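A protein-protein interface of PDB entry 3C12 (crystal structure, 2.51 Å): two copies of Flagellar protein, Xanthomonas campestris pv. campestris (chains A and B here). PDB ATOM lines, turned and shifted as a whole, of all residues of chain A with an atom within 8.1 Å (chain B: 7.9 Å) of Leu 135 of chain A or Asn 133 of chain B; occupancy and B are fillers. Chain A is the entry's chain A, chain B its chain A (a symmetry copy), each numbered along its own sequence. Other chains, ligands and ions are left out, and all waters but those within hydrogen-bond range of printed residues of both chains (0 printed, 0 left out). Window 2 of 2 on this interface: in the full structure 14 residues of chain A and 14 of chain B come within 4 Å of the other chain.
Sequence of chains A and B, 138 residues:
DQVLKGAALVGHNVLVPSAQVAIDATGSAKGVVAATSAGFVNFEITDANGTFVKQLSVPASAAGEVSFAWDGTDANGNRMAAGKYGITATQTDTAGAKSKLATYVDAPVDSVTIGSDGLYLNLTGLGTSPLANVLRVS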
ATOM      1  N   VAL A  14       8.890  -6.203   2.336  1.00  0.00           N
ATOM      2  CA  VAL A  14       7.495  -6.595   2.316  1.00  0.00           C
ATOM      3  C   VAL A  14       7.344  -8.048   1.920  1.00  0.00           C
ATOM      4  O   VAL A  14       8.256  -8.660   1.362  1.00  0.00           O
ATOM      5  CB  VAL A  14       6.678  -5.734   1.321  1.00  0.00           C
ATOM      6  CG1 VAL A  14       6.682  -4.285   1.765  1.00  0.00           C
ATOM      7  CG2 VAL A  14       7.254  -5.867  -0.083  1.00  0.00           C
ATOM      8  N   LEU A  15       6.179  -8.595   2.234  1.00  0.00           N
ATOM      9  CA  LEU A  15       5.866  -9.964   1.897  1.00  0.00           C
ATOM     10  C   LEU A  15       4.737  -9.912   0.902  1.00  0.00           C
ATOM     11  O   LEU A  15       3.657  -9.416   1.199  1.00  0.00           O
ATOM     12  CB  LEU A  15       5.441 -10.749   3.138  1.00  0.00           C
ATOM     13  CG  LEU A  15       6.556 -11.479   3.890  1.00  0.00           C
ATOM     14  CD1 LEU A  15       7.661 -10.510   4.253  1.00  0.00           C
ATOM     15  CD2 LEU A  15       5.983 -12.124   5.130  1.00  0.00           C
ATOM     16  N   VAL A  16       5.006 -10.412  -0.292  1.00  0.00           N
ATOM     17  CA  VAL A  16       4.011 -10.432  -1.343  1.00  0.00           C
ATOM     18  C   VAL A  16       3.906 -11.828  -1.931  1.00  0.00           C
ATOM     19  O   VAL A  16       4.873 -12.587  -1.942  1.00  0.00           O
ATOM     20  CB  VAL A  16       4.378  -9.444  -2.467  1.00  0.00           C
ATOM     21  CG1 VAL A  16       4.343  -8.026  -1.941  1.00  0.00           C
ATOM     22  CG2 VAL A  16       5.761  -9.763  -3.003  1.00  0.00           C
ATOM     23  N   PRO A  17       2.711 -12.193  -2.402  1.00  0.00           N
ATOM     24  CA  PRO A  17       2.477 -13.507  -3.001  1.00  0.00           C
ATOM     25  C   PRO A  17       3.286 -13.597  -4.287  1.00  0.00           C
ATOM     26  O   PRO A  17       3.094 -12.794  -5.195  1.00  0.00           O
ATOM     27  CB  PRO A  17       0.977 -13.498  -3.274  1.00  0.00           C
ATOM     28  CG  PRO A  17       0.449 -12.597  -2.219  1.00  0.00           C
ATOM     29  CD  PRO A  17       1.443 -11.472  -2.222  1.00  0.00           C
ATOM     30  N   VAL A  32       7.825 -16.978   3.274  1.00  0.00           N
ATOM     31  CA  VAL A  32       7.032 -17.779   4.190  1.00  0.00           C
ATOM     32  C   VAL A  32       5.816 -18.385   3.528  1.00  0.00           C
ATOM     33  O   VAL A  32       5.392 -17.965   2.459  1.00  0.00           O
ATOM     34  CB  VAL A  32       6.535 -16.945   5.379  1.00  0.00           C
ATOM     35  CG1 VAL A  32       7.707 -16.453   6.193  1.00  0.00           C
ATOM     36  CG2 VAL A  32       5.721 -15.783   4.877  1.00  0.00           C
ATOM     37  N   ALA A  34       1.912 -20.502   4.742  1.00  0.00           N
ATOM     38  CA  ALA A  34       1.025 -20.814   5.846  1.00  0.00           C
ATOM     39  C   ALA A  34       0.631 -22.283   5.867  1.00  0.00           C
ATOM     40  O   ALA A  34      -0.221 -22.713   5.094  1.00  0.00           O
ATOM     41  CB  ALA A  34      -0.206 -19.939   5.773  1.00  0.00           C
ATOM     42  N   GLU A  65       2.307 -20.260  10.371  1.00  0.00           N
ATOM     43  CA  GLU A  65       3.283 -19.800   9.403  1.00  0.00           C
ATOM     44  C   GLU A  65       4.552 -20.628   9.475  1.00  0.00           C
ATOM     45  O   GLU A  65       4.915 -21.145  10.528  1.00  0.00           O
ATOM     46  CB  GLU A  65       3.614 -18.329   9.663  1.00  0.00           C
ATOM     47  CG  GLU A  65       4.108 -17.569   8.447  1.00  0.00           C
ATOM     48  CD  GLU A  65       4.353 -16.108   8.746  1.00  0.00           C
ATOM     49  OE1 GLU A  65       5.320 -15.806   9.472  1.00  0.00           O
ATOM     50  OE2 GLU A  65       3.574 -15.264   8.262  1.00  0.00           O
ATOM     51  N   ALA A 102       0.370 -21.629  -0.781  1.00  0.00           N
ATOM     52  CA  ALA A 102       0.715 -20.369  -1.439  1.00  0.00           C
ATOM     53  C   ALA A 102       2.009 -19.822  -0.873  1.00  0.00           C
ATOM     54  O   ALA A 102       2.201 -19.795   0.334  1.00  0.00           O
ATOM     55  CB  ALA A 102      -0.391 -19.359  -1.242  1.00  0.00           C
ATOM     56  N   TYR A 104       4.755 -16.768  -0.198  1.00  0.00           N
ATOM     57  CA  TYR A 104       4.869 -15.323  -0.028  1.00  0.00           C
ATOM     58  C   TYR A 104       6.338 -15.017   0.080  1.00  0.00           C
ATOM     59  O   TYR A 104       7.026 -15.510   0.970  1.00  0.00           O
ATOM     60  CB  TYR A 104       4.137 -14.835   1.231  1.00  0.00           C
ATOM     61  CG  TYR A 104       2.665 -15.180   1.229  1.00  0.00           C
ATOM     62  CD1 TYR A 104       2.239 -16.477   1.535  1.00  0.00           C
ATOM     63  CD2 TYR A 104       1.706 -14.244   0.844  1.00  0.00           C
ATOM     64  CE1 TYR A 104       0.892 -16.838   1.450  1.00  0.00           C
ATOM     65  CE2 TYR A 104       0.352 -14.594   0.754  1.00  0.00           C
ATOM     66  CZ  TYR A 104      -0.048 -15.895   1.055  1.00  0.00           C
ATOM     67  OH  TYR A 104      -1.374 -16.277   0.932  1.00  0.00           O
ATOM     68  N   VAL A 105       6.821 -14.201  -0.841  1.00  0.00           N
ATOM     69  CA  VAL A 105       8.228 -13.860  -0.868  1.00  0.00           C
ATOM     70  C   VAL A 105       8.545 -12.544  -0.206  1.00  0.00           C
ATOM     71  O   VAL A 105       7.794 -11.571  -0.332  1.00  0.00           O
ATOM     72  CB  VAL A 105       8.734 -13.798  -2.308  1.00  0.00           C
ATOM     73  CG1 VAL A 105      10.198 -13.445  -2.328  1.00  0.00           C
ATOM     74  CG2 VAL A 105       8.483 -15.117  -2.983  1.00  0.00           C
ATOM     75  N   LEU A 121       4.966  -0.592  -6.144  1.00  0.00           N
ATOM     76  CA  LEU A 121       6.210  -0.781  -5.416  1.00  0.00           C
ATOM     77  C   LEU A 121       7.193  -1.418  -6.368  1.00  0.00           C
ATOM     78  O   LEU A 121       6.840  -2.316  -7.138  1.00  0.00           O
ATOM     79  CB  LEU A 121       6.024  -1.713  -4.221  1.00  0.00           C
ATOM     80  CG  LEU A 121       4.799  -1.539  -3.338  1.00  0.00           C
ATOM     81  CD1 LEU A 121       5.041  -2.278  -2.031  1.00  0.00           C
ATOM     82  CD2 LEU A 121       4.551  -0.068  -3.072  1.00  0.00           C
ATOM     83  N   SER A 129       5.033  -4.451  -8.156  1.00  0.00           N
ATOM     84  CA  SER A 129       3.948  -4.943  -7.356  1.00  0.00           C
ATOM     85  C   SER A 129       3.014  -3.837  -6.947  1.00  0.00           C
ATOM     86  O   SER A 129       3.436  -2.819  -6.416  1.00  0.00           O
ATOM     87  CB  SER A 129       4.464  -5.634  -6.099  1.00  0.00           C
ATOM     88  OG  SER A 129       3.364  -6.060  -5.307  1.00  0.00           O
ATOM     89  N   PRO A 130       1.720  -4.021  -7.206  1.00  0.00           N
ATOM     90  CA  PRO A 130       0.763  -2.989  -6.819  1.00  0.00           C
ATOM     91  C   PRO A 130       0.598  -2.969  -5.295  1.00  0.00           C
ATOM     92  O   PRO A 130       0.516  -4.017  -4.642  1.00  0.00           O
ATOM     93  CB  PRO A 130      -0.511  -3.421  -7.534  1.00  0.00           C
ATOM     94  CG  PRO A 130      -0.374  -4.911  -7.583  1.00  0.00           C
ATOM     95  CD  PRO A 130       1.061  -5.081  -7.986  1.00  0.00           C
ATOM     96  N   ALA A 132      -1.090  -3.332  -2.455  1.00  0.00           N
ATOM     97  CA  ALA A 132      -2.373  -4.016  -2.256  1.00  0.00           C
ATOM     98  C   ALA A 132      -2.061  -5.492  -2.222  1.00  0.00           C
ATOM     99  O   ALA A 132      -2.623  -6.242  -1.419  1.00  0.00           O
ATOM    100  CB  ALA A 132      -3.347  -3.732  -3.406  1.00  0.00           C
ATOM    101  N   ASN A 133      -1.165  -5.900  -3.116  1.00  0.00           N
ATOM    102  CA  ASN A 133      -0.748  -7.281  -3.189  1.00  0.00           C
ATOM    103  C   ASN A 133       0.143  -7.543  -1.999  1.00  0.00           C
ATOM    104  O   ASN A 133       0.538  -8.673  -1.756  1.00  0.00           O
ATOM    105  CB  ASN A 133       0.027  -7.560  -4.477  1.00  0.00           C
ATOM    106  CG  ASN A 133      -0.860  -7.582  -5.705  1.00  0.00           C
ATOM    107  OD1 ASN A 133      -0.587  -8.299  -6.658  1.00  0.00           O
ATOM    108  ND2 ASN A 133      -1.922  -6.788  -5.691  1.00  0.00           N
ATOM    109  N   VAL A 134       0.456  -6.493  -1.246  1.00  0.00           N
ATOM    110  CA  VAL A 134       1.312  -6.655  -0.078  1.00  0.00           C
ATOM    111  C   VAL A 134       0.584  -7.389   1.043  1.00  0.00           C
ATOM    112  O   VAL A 134      -0.567  -7.088   1.355  1.00  0.00           O
ATOM    113  CB  VAL A 134       1.814  -5.300   0.459  1.00  0.00           C
ATOM    114  CG1 VAL A 134       2.826  -5.529   1.586  1.00  0.00           C
ATOM    115  CG2 VAL A 134       2.445  -4.504  -0.667  1.00  0.00           C
ATOM    116  N   LEU A 135       1.266  -8.364   1.636  1.00  0.00           N
ATOM    117  CA  LEU A 135       0.700  -9.148   2.721  1.00  0.00           C
ATOM    118  C   LEU A 135       0.984  -8.453   4.051  1.00  0.00           C
ATOM    119  O   LEU A 135       0.151  -8.461   4.957  1.00  0.00           O
ATOM    120  CB  LEU A 135       1.296 -10.567   2.714  1.00  0.00           C
ATOM    121  CG  LEU A 135       0.828 -11.616   3.748  1.00  0.00           C
ATOM    122  CD1 LEU A 135       1.579 -11.455   5.069  1.00  0.00           C
ATOM    123  CD2 LEU A 135      -0.688 -11.503   3.952  1.00  0.00           C
ATOM    124  N   ARG A 136       2.160  -7.842   4.160  1.00  0.00           N
ATOM    125  CA  ARG A 136       2.542  -7.144   5.374  1.00  0.00           C
ATOM    126  C   ARG A 136       4.004  -6.740   5.302  1.00  0.00           C
ATOM    127  O   ARG A 136       4.764  -7.283   4.501  1.00  0.00           O
ATOM    128  CB  ARG A 136       2.336  -8.036   6.600  1.00  0.00           C
ATOM    129  CG  ARG A 136       3.361  -9.148   6.750  1.00  0.00           C
ATOM    130  CD  ARG A 136       3.387  -9.644   8.180  1.00  0.00           C
ATOM    131  NE  ARG A 136       4.410 -10.657   8.428  1.00  0.00           N
ATOM    132  CZ  ARG A 136       4.195 -11.969   8.387  1.00  0.00           C
ATOM    133  NH1 ARG A 136       2.982 -12.442   8.102  1.00  0.00           N
ATOM    134  NH2 ARG A 136       5.195 -12.807   8.641  1.00  0.00           N
ATOM    135  N   VAL A 137       4.398  -5.796   6.152  1.00  0.00           N
ATOM    136  CA  VAL A 137       5.782  -5.336   6.182  1.00  0.00           C
ATOM    137  C   VAL A 137       6.578  -6.167   7.157  1.00  0.00           C
ATOM    138  O   VAL A 137       6.576  -5.881   8.354  1.00  0.00           O
ATOM    139  CB  VAL A 137       5.914  -3.865   6.650  1.00  0.00           C
ATOM    140  CG1 VAL A 137       7.388  -3.434   6.579  1.00  0.00           C
ATOM    141  CG2 VAL A 137       5.036  -2.957   5.806  1.00  0.00           C
ATOM    142  N   SER A 138       7.255  -7.193   6.656  1.00  0.00           N
ATOM    143  CA  SER A 138       8.074  -8.044   7.525  1.00  0.00           C
ATOM    144  C   SER A 138       9.405  -8.398   6.860  1.00  0.00           C
ATOM    145  O   SER A 138       9.530  -8.151   5.638  1.00  0.00           O
ATOM    146  CB  SER A 138       7.313  -9.337   7.909  1.00  0.00           C
ATOM    147  OG  SER A 138       6.359  -9.118   8.953  1.00  0.00           O
ATOM    148  OXT SER A 138      10.300  -8.923   7.567  1.00  0.00           O
ATOM    149  N   VAL B  14     -14.288 -13.156  -3.270  1.00  0.00           N
ATOM    150  CA  VAL B  14     -13.010 -12.495  -3.103  1.00  0.00           C
ATOM    151  C   VAL B  14     -11.925 -13.206  -3.884  1.00  0.00           C
ATOM    152  O   VAL B  14     -12.075 -14.361  -4.287  1.00  0.00           O
ATOM    153  CB  VAL B  14     -12.584 -12.449  -1.615  1.00  0.00           C
ATOM    154  CG1 VAL B  14     -13.571 -11.619  -0.819  1.00  0.00           C
ATOM    155  CG2 VAL B  14     -12.493 -13.862  -1.051  1.00  0.00           C
ATOM    156  N   LEU B  15     -10.834 -12.488  -4.105  1.00  0.00           N
ATOM    157  CA  LEU B  15      -9.696 -13.031  -4.808  1.00  0.00           C
ATOM    158  C   LEU B  15      -8.566 -13.087  -3.815  1.00  0.00           C
ATOM    159  O   LEU B  15      -8.140 -12.066  -3.287  1.00  0.00           O
ATOM    160  CB  LEU B  15      -9.313 -12.147  -5.995  1.00  0.00           C
ATOM    161  CG  LEU B  15      -9.961 -12.500  -7.336  1.00  0.00           C
ATOM    162  CD1 LEU B  15     -11.468 -12.538  -7.193  1.00  0.00           C
ATOM    163  CD2 LEU B  15      -9.550 -11.481  -8.373  1.00  0.00           C
ATOM    164  N   VAL B  16      -8.097 -14.295  -3.550  1.00  0.00           N
ATOM    165  CA  VAL B  16      -7.008 -14.493  -2.618  1.00  0.00           C
ATOM    166  C   VAL B  16      -5.930 -15.351  -3.257  1.00  0.00           C
ATOM    167  O   VAL B  16      -6.209 -16.188  -4.113  1.00  0.00           O
ATOM    168  CB  VAL B  16      -7.502 -15.187  -1.334  1.00  0.00           C
ATOM    169  CG1 VAL B  16      -8.468 -14.285  -0.598  1.00  0.00           C
ATOM    170  CG2 VAL B  16      -8.181 -16.497  -1.684  1.00  0.00           C
ATOM    171  N   PRO B  17      -4.673 -15.129  -2.863  1.00  0.00           N
ATOM    172  CA  PRO B  17      -3.544 -15.892  -3.393  1.00  0.00           C
ATOM    173  C   PRO B  17      -3.690 -17.338  -2.944  1.00  0.00           C
ATOM    174  O   PRO B  17      -3.726 -17.612  -1.748  1.00  0.00           O
ATOM    175  CB  PRO B  17      -2.339 -15.215  -2.748  1.00  0.00           C
ATOM    176  CG  PRO B  17      -2.803 -13.818  -2.553  1.00  0.00           C
ATOM    177  CD  PRO B  17      -4.201 -14.006  -2.041  1.00  0.00           C
ATOM    178  N   SER B  18      -3.780 -18.261  -3.894  1.00  0.00           N
ATOM    179  CA  SER B  18      -3.931 -19.668  -3.549  1.00  0.00           C
ATOM    180  C   SER B  18      -3.167 -20.553  -4.517  1.00  0.00           C
ATOM    181  O   SER B  18      -3.175 -20.313  -5.717  1.00  0.00           O
ATOM    182  CB  SER B  18      -5.416 -20.049  -3.552  1.00  0.00           C
ATOM    183  OG  SER B  18      -5.611 -21.372  -3.105  1.00  0.00           O
ATOM    184  N   TYR B 104      -4.238 -16.299  -8.193  1.00  0.00           N
ATOM    185  CA  TYR B 104      -5.219 -15.736  -7.270  1.00  0.00           C
ATOM    186  C   TYR B 104      -6.531 -16.405  -7.576  1.00  0.00           C
ATOM    187  O   TYR B 104      -7.041 -16.325  -8.690  1.00  0.00           O
ATOM    188  CB  TYR B 104      -5.354 -14.215  -7.437  1.00  0.00           C
ATOM    189  CG  TYR B 104      -4.050 -13.481  -7.222  1.00  0.00           C
ATOM    190  CD1 TYR B 104      -3.073 -13.460  -8.223  1.00  0.00           C
ATOM    191  CD2 TYR B 104      -3.755 -12.878  -6.000  1.00  0.00           C
ATOM    192  CE1 TYR B 104      -1.827 -12.865  -8.010  1.00  0.00           C
ATOM    193  CE2 TYR B 104      -2.509 -12.278  -5.774  1.00  0.00           C
ATOM    194  CZ  TYR B 104      -1.547 -12.278  -6.783  1.00  0.00           C
ATOM    195  OH  TYR B 104      -0.293 -11.730  -6.569  1.00  0.00           O
ATOM    196  N   TYR B 120     -11.267 -13.747  10.457  1.00  0.00           N
ATOM    197  CA  TYR B 120     -11.017 -14.687   9.371  1.00  0.00           C
ATOM    198  C   TYR B 120     -12.210 -14.922   8.467  1.00  0.00           C
ATOM    199  O   TYR B 120     -13.356 -14.904   8.909  1.00  0.00           O
ATOM    200  CB  TYR B 120     -10.551 -16.026   9.941  1.00  0.00           C
ATOM    201  CG  TYR B 120      -9.221 -15.899  10.632  1.00  0.00           C
ATOM    202  CD1 TYR B 120      -9.133 -15.354  11.920  1.00  0.00           C
ATOM    203  CD2 TYR B 120      -8.032 -16.196   9.949  1.00  0.00           C
ATOM    204  CE1 TYR B 120      -7.889 -15.091  12.512  1.00  0.00           C
ATOM    205  CE2 TYR B 120      -6.784 -15.938  10.523  1.00  0.00           C
ATOM    206  CZ  TYR B 120      -6.718 -15.379  11.806  1.00  0.00           C
ATOM    207  OH  TYR B 120      -5.487 -15.069  12.359  1.00  0.00           O
ATOM    208  N   LEU B 121     -11.932 -15.136   7.186  1.00  0.00           N
ATOM    209  CA  LEU B 121     -12.984 -15.391   6.216  1.00  0.00           C
ATOM    210  C   LEU B 121     -13.047 -16.886   6.009  1.00  0.00           C
ATOM    211  O   LEU B 121     -12.016 -17.559   5.924  1.00  0.00           O
ATOM    212  CB  LEU B 121     -12.680 -14.732   4.873  1.00  0.00           C
ATOM    213  CG  LEU B 121     -12.144 -13.309   4.858  1.00  0.00           C
ATOM    214  CD1 LEU B 121     -12.309 -12.749   3.454  1.00  0.00           C
ATOM    215  CD2 LEU B 121     -12.899 -12.456   5.857  1.00  0.00           C
ATOM    216  N   LEU B 123     -13.875 -19.266   3.455  1.00  0.00           N
ATOM    217  CA  LEU B 123     -14.036 -19.394   2.019  1.00  0.00           C
ATOM    218  C   LEU B 123     -14.551 -20.767   1.632  1.00  0.00           C
ATOM    219  O   LEU B 123     -13.969 -21.789   1.995  1.00  0.00           O
ATOM    220  CB  LEU B 123     -12.701 -19.112   1.347  1.00  0.00           C
ATOM    221  CG  LEU B 123     -12.068 -17.803   1.817  1.00  0.00           C
ATOM    222  CD1 LEU B 123     -10.697 -17.674   1.198  1.00  0.00           C
ATOM    223  CD2 LEU B 123     -12.950 -16.609   1.440  1.00  0.00           C
ATOM    224  N   THR B 128      -9.960 -21.496   5.142  1.00  0.00           N
ATOM    225  CA  THR B 128      -9.789 -20.261   5.877  1.00  0.00           C
ATOM    226  C   THR B 128      -8.836 -19.267   5.262  1.00  0.00           C
ATOM    227  O   THR B 128      -7.888 -19.626   4.565  1.00  0.00           O
ATOM    228  CB  THR B 128      -9.333 -20.550   7.323  1.00  0.00           C
ATOM    229  OG1 THR B 128     -10.416 -20.252   8.216  1.00  0.00           O
ATOM    230  CG2 THR B 128      -8.073 -19.730   7.692  1.00  0.00           C
ATOM    231  N   SER B 129      -9.097 -18.000   5.541  1.00  0.00           N
ATOM    232  CA  SER B 129      -8.252 -16.953   5.043  1.00  0.00           C
ATOM    233  C   SER B 129      -8.326 -15.723   5.905  1.00  0.00           C
ATOM    234  O   SER B 129      -9.403 -15.222   6.199  1.00  0.00           O
ATOM    235  CB  SER B 129      -8.634 -16.572   3.617  1.00  0.00           C
ATOM    236  OG  SER B 129      -7.813 -15.499   3.177  1.00  0.00           O
ATOM    237  N   PRO B 130      -7.168 -15.223   6.336  1.00  0.00           N
ATOM    238  CA  PRO B 130      -7.175 -14.021   7.164  1.00  0.00           C
ATOM    239  C   PRO B 130      -7.546 -12.799   6.315  1.00  0.00           C
ATOM    240  O   PRO B 130      -7.081 -12.638   5.179  1.00  0.00           O
ATOM    241  CB  PRO B 130      -5.744 -13.956   7.680  1.00  0.00           C
ATOM    242  CG  PRO B 130      -4.963 -14.592   6.572  1.00  0.00           C
ATOM    243  CD  PRO B 130      -5.811 -15.783   6.234  1.00  0.00           C
ATOM    244  N   LEU B 131      -8.424 -11.967   6.855  1.00  0.00           N
ATOM    245  CA  LEU B 131      -8.825 -10.749   6.175  1.00  0.00           C
ATOM    246  C   LEU B 131      -7.492 -10.018   6.091  1.00  0.00           C
ATOM    247  O   LEU B 131      -6.932  -9.637   7.125  1.00  0.00           O
ATOM    248  CB  LEU B 131      -9.809  -9.980   7.063  1.00  0.00           C
ATOM    249  CG  LEU B 131     -10.449  -8.692   6.551  1.00  0.00           C
ATOM    250  CD1 LEU B 131      -9.422  -7.566   6.548  1.00  0.00           C
ATOM    251  CD2 LEU B 131     -11.025  -8.945   5.160  1.00  0.00           C
ATOM    252  N   ALA B 132      -6.970  -9.859   4.878  1.00  0.00           N
ATOM    253  CA  ALA B 132      -5.675  -9.204   4.662  1.00  0.00           C
ATOM    254  C   ALA B 132      -5.059  -9.877   3.460  1.00  0.00           C
ATOM    255  O   ALA B 132      -4.456  -9.222   2.605  1.00  0.00           O
ATOM    256  CB  ALA B 132      -4.746  -9.383   5.870  1.00  0.00           C
ATOM    257  N   ASN B 133      -5.210 -11.197   3.413  1.00  0.00           N
ATOM    258  CA  ASN B 133      -4.694 -11.976   2.312  1.00  0.00           C
ATOM    259  C   ASN B 133      -5.586 -11.713   1.122  1.00  0.00           C
ATOM    260  O   ASN B 133      -5.301 -12.160   0.021  1.00  0.00           O
ATOM    261  CB  ASN B 133      -4.704 -13.470   2.635  1.00  0.00           C
ATOM    262  CG  ASN B 133      -3.639 -13.864   3.637  1.00  0.00           C
ATOM    263  OD1 ASN B 133      -3.124 -14.972   3.596  1.00  0.00           O
ATOM    264  ND2 ASN B 133      -3.310 -12.957   4.548  1.00  0.00           N
ATOM    265  N   VAL B 134      -6.670 -10.976   1.342  1.00  0.00           N
ATOM    266  CA  VAL B 134      -7.587 -10.673   0.249  1.00  0.00           C
ATOM    267  C   VAL B 134      -6.970  -9.683  -0.732  1.00  0.00           C
ATOM    268  O   VAL B 134      -6.382  -8.679  -0.334  1.00  0.00           O
ATOM    269  CB  VAL B 134      -8.922 -10.098   0.762  1.00  0.00           C
ATOM    270  CG1 VAL B 134      -9.904  -9.940  -0.403  1.00  0.00           C
ATOM    271  CG2 VAL B 134      -9.501 -11.014   1.823  1.00  0.00           C
ATOM    272  N   LEU B 135      -7.101  -9.985  -2.020  1.00  0.00           N
ATOM    273  CA  LEU B 135      -6.563  -9.133  -3.068  1.00  0.00           C
ATOM    274  C   LEU B 135      -7.602  -8.080  -3.446  1.00  0.00           C
ATOM    275  O   LEU B 135      -7.261  -6.932  -3.733  1.00  0.00           O
ATOM    276  CB  LEU B 135      -6.181  -9.982  -4.294  1.00  0.00           C
ATOM    277  CG  LEU B 135      -5.547  -9.317  -5.537  1.00  0.00           C
ATOM    278  CD1 LEU B 135      -6.622  -8.728  -6.450  1.00  0.00           C
ATOM    279  CD2 LEU B 135      -4.544  -8.245  -5.096  1.00  0.00           C
ATOM    280  N   ARG B 136      -8.873  -8.471  -3.436  1.00  0.00           N
ATOM    281  CA  ARG B 136      -9.950  -7.558  -3.774  1.00  0.00           C
ATOM    282  C   ARG B 136     -11.257  -8.321  -3.897  1.00  0.00           C
ATOM    283  O   ARG B 136     -11.257  -9.542  -4.055  1.00  0.00           O
ATOM    284  CB  ARG B 136      -9.665  -6.850  -5.100  1.00  0.00           C
ATOM    285  CG  ARG B 136      -9.832  -7.725  -6.331  1.00  0.00           C
ATOM    286  CD  ARG B 136     -10.016  -6.864  -7.562  1.00  0.00           C
ATOM    287  NE  ARG B 136     -10.271  -7.631  -8.779  1.00  0.00           N
ATOM    288  CZ  ARG B 136      -9.332  -7.995  -9.649  1.00  0.00           C
ATOM    289  NH1 ARG B 136      -8.058  -7.663  -9.441  1.00  0.00           N
ATOM    290  NH2 ARG B 136      -9.674  -8.683 -10.734  1.00  0.00           N
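The side-chain hydroxyl of Tyr 104 of chain A is in hydrogen-bond range of the side-chain amide oxygen of Asn 133 of chain B, 3.4 Å away.
The side-chain hydroxyl (OH) of Tyr 104 of chain B lies within hydrogen-bond range of the side-chain amide oxygen (OD1) of Asn 133 of chain A.
N of Leu 135 of chain B is in hydrogen-bond range of O of Leu 15 of chain B (2.6 Å).
The backbone NH (N) of Val 32 of chain A lies within hydrogen-bond range of the backbone carbonyl oxygen (O) of Tyr 104 of chain A, 2.8 Å away.
N of Leu 135 of chain A is in hydrogen-bond range of O of Leu 15 of chain A, 2.6 Å away.
Pro 17 of chain A touches Pro 17 of chain B.
O of Pro 17 of chain A touches OH of Tyr 104 of chain B, at 3.8 Å.
Ala 102 of chain A touches Pro 17 of chain B.
O of Pro 17 of chain B touches OH of Tyr 104 of chain A (3.8 Å).
Leu 135 of chain B touches Asn 133 of chain A.
Asn 133 of chain B touches Leu 135 of chain A.
Val 16 of chain A touches none of the printed residues of chain B.
Printed residues of chain B within 4 Å of Pro 17 of chain A: Pro 17 (3.5 Å) and Tyr 104 (3.8 Å).
Ala 34 of chain A touches none of the printed residues of chain B.
Of the printed residues of chain B, Tyr 104 of chain A touches Pro 17 (3.8 Å) and Asn 133 (3.4 Å).
Printed residues of chain B within 4 Å of Asn 133 of chain A: Tyr 104 (3.4 Å) and Leu 135 (3.1 Å).
Of the printed residues of chain A, Tyr 104 of chain B touches Pro 17 (3.8 Å) and Asn 133 (3.4 Å).
No residue of chain A comes within 4 Å of Ala 132 of chain B.
Of the printed residues of chain A, Leu 135 of chain B touches Asn 133 (3.1 Å).
The nearest residue of chain B that does not touch Leu 135 of chain A is Ala 132 of chain B (4.6 Å).
The nearest printed residue of chain A that does not touch Asn 133 of chain B is Ala 34 of chain A (6.2 Å).
Of the 18 printed residues of chain B, 4 touch a printed residue of chain A.
Hydrophobic or aromatic side chains of chain B that line the printed part of chain A: Pro 17, Tyr 104 and Leu 135.
Of the 20 printed residues of chain A, 5 touch a printed residue of chain B.
Hydrophobic or aromatic side chains of chain A within 4 Å of the printed part of chain B: Pro 17, Ala 102, Tyr 104 and Leu 135.
Along chain A the printed residues that touch a printed residue of chain B span positions 17 to 135.
Among the printed residues, 8 pairs touch across the chains.
Among the printed residues, no Asp or Glu carboxylate lies within 4 Å of a Lys or Arg side-chain nitrogen of the other chain.
Pro 17 of chain B touches its own counterpart, Pro 17 of chain A.
Pro 17 of chain A touches Tyr 104 of chain B, and with the chains exchanged Tyr 104 of chain A touches Pro 17 of chain B.
Tyr 104 of chain A touches Asn 133 of chain B, and with the chains exchanged Asn 133 of chain A touches Tyr 104 of chain B.
Asn 133 of chain A touches Leu 135 of chain B, and with the chains exchanged Leu 135 of chain A touches Asn 133 of chain B.
13 positions are printed for both chains.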
